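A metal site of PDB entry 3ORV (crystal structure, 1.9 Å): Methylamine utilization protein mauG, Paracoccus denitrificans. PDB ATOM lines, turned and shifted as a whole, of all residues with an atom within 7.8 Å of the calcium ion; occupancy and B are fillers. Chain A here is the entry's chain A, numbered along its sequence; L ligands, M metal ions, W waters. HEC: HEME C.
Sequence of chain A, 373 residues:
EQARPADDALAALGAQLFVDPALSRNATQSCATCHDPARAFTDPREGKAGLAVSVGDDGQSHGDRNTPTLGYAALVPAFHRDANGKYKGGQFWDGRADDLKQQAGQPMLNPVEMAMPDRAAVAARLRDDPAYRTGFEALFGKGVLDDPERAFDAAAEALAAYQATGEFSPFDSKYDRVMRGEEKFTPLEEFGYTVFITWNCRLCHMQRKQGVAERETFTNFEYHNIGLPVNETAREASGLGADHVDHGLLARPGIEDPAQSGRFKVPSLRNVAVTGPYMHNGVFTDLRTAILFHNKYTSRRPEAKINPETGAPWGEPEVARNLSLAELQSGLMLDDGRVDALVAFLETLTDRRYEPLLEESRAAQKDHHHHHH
A ring nitrogen (ND1) of His 280 lies within hydrogen-bond range of an oxygen (O2D) of the ligand (2.7 Å).
N of His 280 lies within hydrogen-bond range of O1D of the ligand, 2.7 Å away.
The backbone NH (N) of Met 279 lies within hydrogen-bond range of an oxygen (O1A) of the ligand (2.9 Å).
The backbone carbonyl oxygen (O) of Asn 66 sits at hydrogen-bond distance from the indole nitrogen (NE1) of Trp 93 (2.8 Å).
The side-chain amide nitrogen of Asn 66 sits at hydrogen-bond distance from the backbone carbonyl oxygen of Leu 51 (3.2 Å).
The side-chain hydroxyl (OG1) of Thr 275 sits close to the backbone carbonyl oxygen (O) of Val 272 (3.5 Å).
O of His 280 sits at hydrogen-bond distance from N of Asn 66, 2.6 Å away.
The backbone carbonyl oxygen (O) of Ala 52 sits at hydrogen-bond distance from the side-chain amide nitrogen (ND2) of Asn 66.
Of the 21 residues printed, 3 come within 4 Å of the calcium ion.
Along chain A the residues within 4 Å of the calcium ion span positions 66 to 277.
The nearest printed residue that does not touch the calcium ion is Gly 276 (4.2 Å).
The calcium ion is bound by water W1 (2.2 Å), O of Thr 275 (2.4 Å), OD1 of Asn 66 (2.4 Å), O of Pro 277 (2.5 Å), water W4 (2.5 Å), water W2 (2.5 Å) and water W3 (2.5 Å).
Water W2 bridges OG1 of Thr 275 (2.7 Å) and O2A of the ligand (2.8 Å).
Water W4 bridges ND2 of Asn 66 (3.1 Å) and O of Gly 276 (3.2 Å).
Water W3 bridges O1A of the ligand and O of Met 279.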
ATOM      1  N   ARG A  39     -18.584 -18.878  23.057  1.00  0.00           N
ATOM      2  CA  ARG A  39     -18.598 -18.834  21.574  1.00  0.00           C
ATOM      3  C   ARG A  39     -19.946 -19.270  20.980  1.00  0.00           C
ATOM      4  O   ARG A  39     -19.986 -19.992  20.001  1.00  0.00           O
ATOM      5  CB  ARG A  39     -17.433 -19.619  20.918  1.00  0.00           C
ATOM      6  CG  ARG A  39     -17.054 -19.045  19.453  1.00  0.00           C
ATOM      7  CD  ARG A  39     -15.589 -19.267  18.906  1.00  0.00           C
ATOM      8  NE  ARG A  39     -15.883 -20.195  17.909  1.00  0.00           N
ATOM      9  CZ  ARG A  39     -15.945 -20.201  16.573  1.00  0.00           C
ATOM     10  NH1 ARG A  39     -15.245 -19.495  15.647  1.00  0.00           N
ATOM     11  NH2 ARG A  39     -16.687 -21.210  16.188  1.00  0.00           N
ATOM     12  N   THR A  42     -20.319 -23.150  20.460  1.00  0.00           N
ATOM     13  CA  THR A  42     -19.561 -23.903  19.448  1.00  0.00           C
ATOM     14  C   THR A  42     -18.099 -23.969  19.864  1.00  0.00           C
ATOM     15  O   THR A  42     -17.729 -23.497  20.981  1.00  0.00           O
ATOM     16  CB  THR A  42     -19.667 -23.201  18.082  1.00  0.00           C
ATOM     17  OG1 THR A  42     -19.042 -21.906  18.187  1.00  0.00           O
ATOM     18  CG2 THR A  42     -21.219 -23.050  17.677  1.00  0.00           C
ATOM     19  N   ASP A  43     -17.255 -24.507  18.971  1.00  0.00           N
ATOM     20  CA  ASP A  43     -15.903 -24.958  19.390  1.00  0.00           C
ATOM     21  C   ASP A  43     -14.802 -24.027  18.818  1.00  0.00           C
ATOM     22  O   ASP A  43     -14.552 -24.024  17.622  1.00  0.00           O
ATOM     23  CB  ASP A  43     -15.676 -26.429  18.934  1.00  0.00           C
ATOM     24  CG  ASP A  43     -14.419 -27.056  19.574  1.00  0.00           C
ATOM     25  OD1 ASP A  43     -14.178 -28.234  19.231  1.00  0.00           O
ATOM     26  OD2 ASP A  43     -13.668 -26.382  20.365  1.00  0.00           O
ATOM     27  N   LEU A  51     -10.915 -25.178  12.518  1.00  0.00           N
ATOM     28  CA  LEU A  51     -12.123 -25.220  13.311  1.00  0.00           C
ATOM     29  C   LEU A  51     -13.232 -26.046  12.652  1.00  0.00           C
ATOM     30  O   LEU A  51     -14.382 -26.075  13.182  1.00  0.00           O
ATOM     31  CB  LEU A  51     -12.642 -23.795  13.625  1.00  0.00           C
ATOM     32  CG  LEU A  51     -12.060 -23.174  14.905  1.00  0.00           C
ATOM     33  CD1 LEU A  51     -10.561 -23.047  14.761  1.00  0.00           C
ATOM     34  CD2 LEU A  51     -12.701 -21.825  15.218  1.00  0.00           C
ATOM     35  N   ALA A  52     -12.889 -26.757  11.564  1.00  0.00           N
ATOM     36  CA  ALA A  52     -13.868 -27.522  10.795  1.00  0.00           C
ATOM     37  C   ALA A  52     -14.499 -28.626  11.660  1.00  0.00           C
ATOM     38  O   ALA A  52     -15.705 -28.782  11.614  1.00  0.00           O
ATOM     39  CB  ALA A  52     -13.276 -28.124   9.531  1.00  0.00           C
ATOM     40  N   ASN A  66     -19.039 -30.458  11.541  1.00  0.00           N
ATOM     41  CA  ASN A  66     -18.776 -29.241  12.356  1.00  0.00           C
ATOM     42  C   ASN A  66     -19.699 -29.214  13.574  1.00  0.00           C
ATOM     43  O   ASN A  66     -20.897 -29.527  13.460  1.00  0.00           O
ATOM     44  CB  ASN A  66     -19.022 -28.025  11.435  1.00  0.00           C
ATOM     45  CG  ASN A  66     -18.750 -26.733  12.098  1.00  0.00           C
ATOM     46  OD1 ASN A  66     -19.660 -25.940  12.283  1.00  0.00           O
ATOM     47  ND2 ASN A  66     -17.468 -26.500  12.461  1.00  0.00           N
ATOM     48  N   THR A  67     -19.186 -28.839  14.745  1.00  0.00           N
ATOM     49  CA  THR A  67     -19.995 -28.771  15.962  1.00  0.00           C
ATOM     50  C   THR A  67     -20.973 -27.581  15.866  1.00  0.00           C
ATOM     51  O   THR A  67     -20.509 -26.426  15.696  1.00  0.00           O
ATOM     52  CB  THR A  67     -19.106 -28.547  17.195  1.00  0.00           C
ATOM     53  OG1 THR A  67     -18.301 -29.692  17.390  1.00  0.00           O
ATOM     54  CG2 THR A  67     -19.918 -28.271  18.466  1.00  0.00           C
ATOM     55  N   PRO A  68     -22.283 -27.817  15.961  1.00  0.00           N
ATOM     56  CA  PRO A  68     -23.225 -26.684  15.780  1.00  0.00           C
ATOM     57  C   PRO A  68     -23.513 -25.950  17.108  1.00  0.00           C
ATOM     58  O   PRO A  68     -23.340 -26.526  18.224  1.00  0.00           O
ATOM     59  CB  PRO A  68     -24.474 -27.387  15.198  1.00  0.00           C
ATOM     60  CG  PRO A  68     -24.474 -28.749  16.011  1.00  0.00           C
ATOM     61  CD  PRO A  68     -22.996 -29.131  16.012  1.00  0.00           C
ATOM     62  N   THR A  69     -23.984 -24.723  17.024  1.00  0.00           N
ATOM     63  CA  THR A  69     -24.627 -24.086  18.204  1.00  0.00           C
ATOM     64  C   THR A  69     -25.731 -24.839  18.900  1.00  0.00           C
ATOM     65  O   THR A  69     -26.568 -25.533  18.274  1.00  0.00           O
ATOM     66  CB  THR A  69     -25.079 -22.590  17.887  1.00  0.00           C
ATOM     67  OG1 THR A  69     -25.378 -21.912  19.104  1.00  0.00           O
ATOM     68  CG2 THR A  69     -26.334 -22.544  16.969  1.00  0.00           C
ATOM     69  N   TRP A  93     -26.987 -32.828  12.450  1.00  0.00           N
ATOM     70  CA  TRP A  93     -27.095 -32.314  11.100  1.00  0.00           C
ATOM     71  C   TRP A  93     -27.907 -33.291  10.253  1.00  0.00           C
ATOM     72  O   TRP A  93     -28.441 -32.878   9.259  1.00  0.00           O
ATOM     73  CB  TRP A  93     -25.690 -32.189  10.496  1.00  0.00           C
ATOM     74  CG  TRP A  93     -24.836 -30.995  10.988  1.00  0.00           C
ATOM     75  CD1 TRP A  93     -23.848 -31.001  11.929  1.00  0.00           C
ATOM     76  CD2 TRP A  93     -24.888 -29.643  10.480  1.00  0.00           C
ATOM     77  NE1 TRP A  93     -23.289 -29.728  12.085  1.00  0.00           N
ATOM     78  CE2 TRP A  93     -23.902 -28.885  11.182  1.00  0.00           C
ATOM     79  CE3 TRP A  93     -25.636 -29.020   9.473  1.00  0.00           C
ATOM     80  CZ2 TRP A  93     -23.677 -27.536  10.930  1.00  0.00           C
ATOM     81  CZ3 TRP A  93     -25.418 -27.635   9.218  1.00  0.00           C
ATOM     82  CH2 TRP A  93     -24.422 -26.918   9.911  1.00  0.00           C
ATOM     83  N   VAL A 272     -24.966 -16.809  13.534  1.00  0.00           N
ATOM     84  CA  VAL A 272     -24.152 -17.363  12.490  1.00  0.00           C
ATOM     85  C   VAL A 272     -22.846 -16.546  12.321  1.00  0.00           C
ATOM     86  O   VAL A 272     -21.805 -17.086  11.905  1.00  0.00           O
ATOM     87  CB  VAL A 272     -24.968 -17.427  11.127  1.00  0.00           C
ATOM     88  CG1 VAL A 272     -25.307 -16.031  10.563  1.00  0.00           C
ATOM     89  CG2 VAL A 272     -24.252 -18.244  10.087  1.00  0.00           C
ATOM     90  N   VAL A 274     -20.872 -15.437  14.444  1.00  0.00           N
ATOM     91  CA  VAL A 274     -19.821 -15.748  15.382  1.00  0.00           C
ATOM     92  C   VAL A 274     -19.582 -17.272  15.480  1.00  0.00           C
ATOM     93  O   VAL A 274     -18.828 -17.747  16.379  1.00  0.00           O
ATOM     94  CB  VAL A 274     -20.132 -15.092  16.782  1.00  0.00           C
ATOM     95  CG1 VAL A 274     -20.287 -13.596  16.629  1.00  0.00           C
ATOM     96  CG2 VAL A 274     -21.385 -15.780  17.452  1.00  0.00           C
ATOM     97  N   THR A 275     -20.225 -18.065  14.602  1.00  0.00           N
ATOM     98  CA  THR A 275     -20.083 -19.545  14.697  1.00  0.00           C
ATOM     99  C   THR A 275     -19.362 -20.171  13.481  1.00  0.00           C
ATOM    100  O   THR A 275     -19.550 -21.361  13.221  1.00  0.00           O
ATOM    101  CB  THR A 275     -21.471 -20.262  14.919  1.00  0.00           C
ATOM    102  OG1 THR A 275     -22.336 -19.937  13.802  1.00  0.00           O
ATOM    103  CG2 THR A 275     -22.127 -19.827  16.191  1.00  0.00           C
ATOM    104  N   GLY A 276     -18.525 -19.416  12.771  1.00  0.00           N
ATOM    105  CA  GLY A 276     -17.756 -20.033  11.690  1.00  0.00           C
ATOM    106  C   GLY A 276     -16.792 -21.091  12.184  1.00  0.00           C
ATOM    107  O   GLY A 276     -16.504 -21.107  13.375  1.00  0.00           O
ATOM    108  N   PRO A 277     -16.263 -21.946  11.278  1.00  0.00           N
ATOM    109  CA  PRO A 277     -16.488 -22.024   9.828  1.00  0.00           C
ATOM    110  C   PRO A 277     -17.891 -22.595   9.564  1.00  0.00           C
ATOM    111  O   PRO A 277     -18.560 -23.001  10.524  1.00  0.00           O
ATOM    112  CB  PRO A 277     -15.362 -22.960   9.377  1.00  0.00           C
ATOM    113  CG  PRO A 277     -15.145 -23.873  10.524  1.00  0.00           C
ATOM    114  CD  PRO A 277     -15.286 -22.936  11.736  1.00  0.00           C
ATOM    115  N   TYR A 278     -18.298 -22.738   8.284  1.00  0.00           N
ATOM    116  CA  TYR A 278     -19.677 -22.966   8.009  1.00  0.00           C
ATOM    117  C   TYR A 278     -19.951 -24.276   7.258  1.00  0.00           C
ATOM    118  O   TYR A 278     -19.049 -24.845   6.704  1.00  0.00           O
ATOM    119  CB  TYR A 278     -20.160 -21.738   7.203  1.00  0.00           C
ATOM    120  CG  TYR A 278     -20.042 -20.496   8.030  1.00  0.00           C
ATOM    121  CD1 TYR A 278     -19.030 -19.551   7.757  1.00  0.00           C
ATOM    122  CD2 TYR A 278     -20.874 -20.307   9.145  1.00  0.00           C
ATOM    123  CE1 TYR A 278     -18.871 -18.466   8.546  1.00  0.00           C
ATOM    124  CE2 TYR A 278     -20.778 -19.129   9.916  1.00  0.00           C
ATOM    125  CZ  TYR A 278     -19.778 -18.251   9.616  1.00  0.00           C
ATOM    126  OH  TYR A 278     -19.634 -17.096  10.378  1.00  0.00           O
ATOM    127  N   MET A 279     -21.227 -24.678   7.232  1.00  0.00           N
ATOM    128  CA  MET A 279     -21.697 -25.934   6.642  1.00  0.00           C
ATOM    129  C   MET A 279     -21.434 -27.105   7.585  1.00  0.00           C
ATOM    130  O   MET A 279     -20.728 -26.945   8.583  1.00  0.00           O
ATOM    131  CB  MET A 279     -21.063 -26.177   5.267  1.00  0.00           C
ATOM    132  CG  MET A 279     -21.327 -24.986   4.274  1.00  0.00           C
ATOM    133  SD  MET A 279     -23.079 -24.522   4.251  1.00  0.00           S
ATOM    134  CE  MET A 279     -22.956 -22.991   3.324  1.00  0.00           C
ATOM    135  N   HIS A 280     -22.054 -28.260   7.265  1.00  0.00           N
ATOM    136  CA  HIS A 280     -22.033 -29.443   8.118  1.00  0.00           C
ATOM    137  C   HIS A 280     -20.579 -29.995   8.241  1.00  0.00           C
ATOM    138  O   HIS A 280     -20.281 -30.722   9.217  1.00  0.00           O
ATOM    139  CB  HIS A 280     -22.955 -30.537   7.548  1.00  0.00           C
ATOM    140  CG  HIS A 280     -22.472 -31.119   6.249  1.00  0.00           C
ATOM    141  ND1 HIS A 280     -23.048 -30.818   5.018  1.00  0.00           N
ATOM    142  CD2 HIS A 280     -21.458 -31.997   5.984  1.00  0.00           C
ATOM    143  CE1 HIS A 280     -22.420 -31.481   4.053  1.00  0.00           C
ATOM    144  NE2 HIS A 280     -21.434 -32.191   4.613  1.00  0.00           N
ATOM    145  N   ASN A 281     -19.715 -29.659   7.311  1.00  0.00           N
ATOM    146  CA  ASN A 281     -18.307 -30.072   7.374  1.00  0.00           C
ATOM    147  C   ASN A 281     -17.329 -28.919   7.539  1.00  0.00           C
ATOM    148  O   ASN A 281     -16.111 -29.118   7.379  1.00  0.00           O
ATOM    149  CB  ASN A 281     -17.950 -30.903   6.147  1.00  0.00           C
ATOM    150  CG  ASN A 281     -18.184 -30.136   4.856  1.00  0.00           C
ATOM    151  OD1 ASN A 281     -18.381 -28.910   4.892  1.00  0.00           O
ATOM    152  ND2 ASN A 281     -18.192 -30.840   3.709  1.00  0.00           N
ATOM    153  N   GLY A 282     -17.823 -27.731   7.906  1.00  0.00           N
ATOM    154  CA  GLY A 282     -16.888 -26.650   8.278  1.00  0.00           C
ATOM    155  C   GLY A 282     -16.024 -26.186   7.121  1.00  0.00           C
ATOM    156  O   GLY A 282     -14.953 -25.626   7.337  1.00  0.00           O
ATOM    157  N   PHE A 284     -16.159 -23.858   4.724  1.00  0.00           N
ATOM    158  CA  PHE A 284     -15.883 -22.466   4.376  1.00  0.00           C
ATOM    159  C   PHE A 284     -15.631 -21.669   5.657  1.00  0.00           C
ATOM    160  O   PHE A 284     -16.440 -21.738   6.587  1.00  0.00           O
ATOM    161  CB  PHE A 284     -17.095 -21.866   3.632  1.00  0.00           C
ATOM    162  CG  PHE A 284     -17.510 -22.647   2.442  1.00  0.00           C
ATOM    163  CD1 PHE A 284     -16.592 -23.017   1.463  1.00  0.00           C
ATOM    164  CD2 PHE A 284     -18.873 -22.922   2.240  1.00  0.00           C
ATOM    165  CE1 PHE A 284     -17.027 -23.757   0.361  1.00  0.00           C
ATOM    166  CE2 PHE A 284     -19.292 -23.630   1.159  1.00  0.00           C
ATOM    167  CZ  PHE A 284     -18.394 -24.044   0.212  1.00  0.00           C
HETATM  168 FE   HEC L   1     -28.660 -21.469   3.353  1.00  0.00          FE
HETATM  169  CHA HEC L   1     -26.361 -23.179   5.289  1.00  0.00           C
HETATM  170  CHB HEC L   1     -27.373 -18.526   4.403  1.00  0.00           C
HETATM  171  CHC HEC L   1     -30.421 -19.914   0.975  1.00  0.00           C
HETATM  172  CHD HEC L   1     -30.427 -24.351   2.937  1.00  0.00           C
HETATM  173  NA  HEC L   1     -27.111 -20.938   4.682  1.00  0.00           N
HETATM  174  C1A HEC L   1     -26.248 -21.720   5.327  1.00  0.00           C
HETATM  175  C2A HEC L   1     -25.237 -20.977   6.082  1.00  0.00           C
HETATM  176  C3A HEC L   1     -25.531 -19.637   5.826  1.00  0.00           C
HETATM  177  C4A HEC L   1     -26.686 -19.709   4.931  1.00  0.00           C
HETATM  178  CMA HEC L   1     -24.868 -18.356   6.257  1.00  0.00           C
HETATM  179  CAA HEC L   1     -24.135 -21.520   6.958  1.00  0.00           C
HETATM  180  CBA HEC L   1     -24.895 -21.758   8.305  1.00  0.00           C
HETATM  181  CGA HEC L   1     -24.043 -22.505   9.322  1.00  0.00           C
HETATM  182  O1A HEC L   1     -23.095 -23.167   8.909  1.00  0.00           O
HETATM  183  O2A HEC L   1     -24.409 -22.625  10.498  1.00  0.00           O
HETATM  184  NB  HEC L   1     -28.852 -19.526   2.767  1.00  0.00           N
HETATM  185  C1B HEC L   1     -28.317 -18.469   3.305  1.00  0.00           C
HETATM  186  C2B HEC L   1     -28.741 -17.217   2.685  1.00  0.00           C
HETATM  187  C3B HEC L   1     -29.593 -17.603   1.704  1.00  0.00           C
HETATM  188  C4B HEC L   1     -29.647 -19.072   1.836  1.00  0.00           C
HETATM  189  CMB HEC L   1     -28.297 -15.794   3.031  1.00  0.00           C
HETATM  190  CAB HEC L   1     -30.302 -16.792   0.658  1.00  0.00           C
HETATM  191  CBB HEC L   1     -29.221 -16.167  -0.262  1.00  0.00           C
HETATM  192  NC  HEC L   1     -30.183 -22.055   2.103  1.00  0.00           N
HETATM  193  C1C HEC L   1     -30.818 -21.314   1.235  1.00  0.00           C
HETATM  194  C2C HEC L   1     -31.892 -22.004   0.552  1.00  0.00           C
HETATM  195  C3C HEC L   1     -31.933 -23.265   1.149  1.00  0.00           C
HETATM  196  C4C HEC L   1     -30.800 -23.219   2.090  1.00  0.00           C
HETATM  197  CMC HEC L   1     -32.784 -21.384  -0.502  1.00  0.00           C
HETATM  198  CAC HEC L   1     -32.822 -24.482   0.922  1.00  0.00           C
HETATM  199  CBC HEC L   1     -32.679 -24.983  -0.525  1.00  0.00           C
HETATM  200  ND  HEC L   1     -28.439 -23.434   3.980  1.00  0.00           N
HETATM  201  C1D HEC L   1     -29.201 -24.475   3.693  1.00  0.00           C
HETATM  202  C2D HEC L   1     -28.731 -25.744   4.252  1.00  0.00           C
HETATM  203  C3D HEC L   1     -27.568 -25.403   4.863  1.00  0.00           C
HETATM  204  C4D HEC L   1     -27.445 -23.952   4.715  1.00  0.00           C
HETATM  205  CMD HEC L   1     -29.344 -27.106   4.101  1.00  0.00           C
HETATM  206  CAD HEC L   1     -26.626 -26.367   5.539  1.00  0.00           C
HETATM  207  CBD HEC L   1     -25.929 -27.045   4.303  1.00  0.00           C
HETATM  208  CGD HEC L   1     -25.028 -28.150   4.812  1.00  0.00           C
HETATM  209  O1D HEC L   1     -24.230 -27.853   5.735  1.00  0.00           O
HETATM  210  O2D HEC L   1     -25.157 -29.317   4.331  1.00  0.00           O
HETATM  211 CA    CA M   1     -20.131 -23.553  12.349  1.00  0.00          CA
HETATM  212  O   HOH W   1     -21.244 -24.135  14.183  1.00  0.00           O
HETATM  213  O   HOH W   2     -22.096 -22.022  12.034  1.00  0.00           O
HETATM  214  O   HOH W   3     -21.525 -24.701  10.587  1.00  0.00           O
HETATM  215  O   HOH W   4     -18.094 -23.803  13.790  1.00  0.00           O
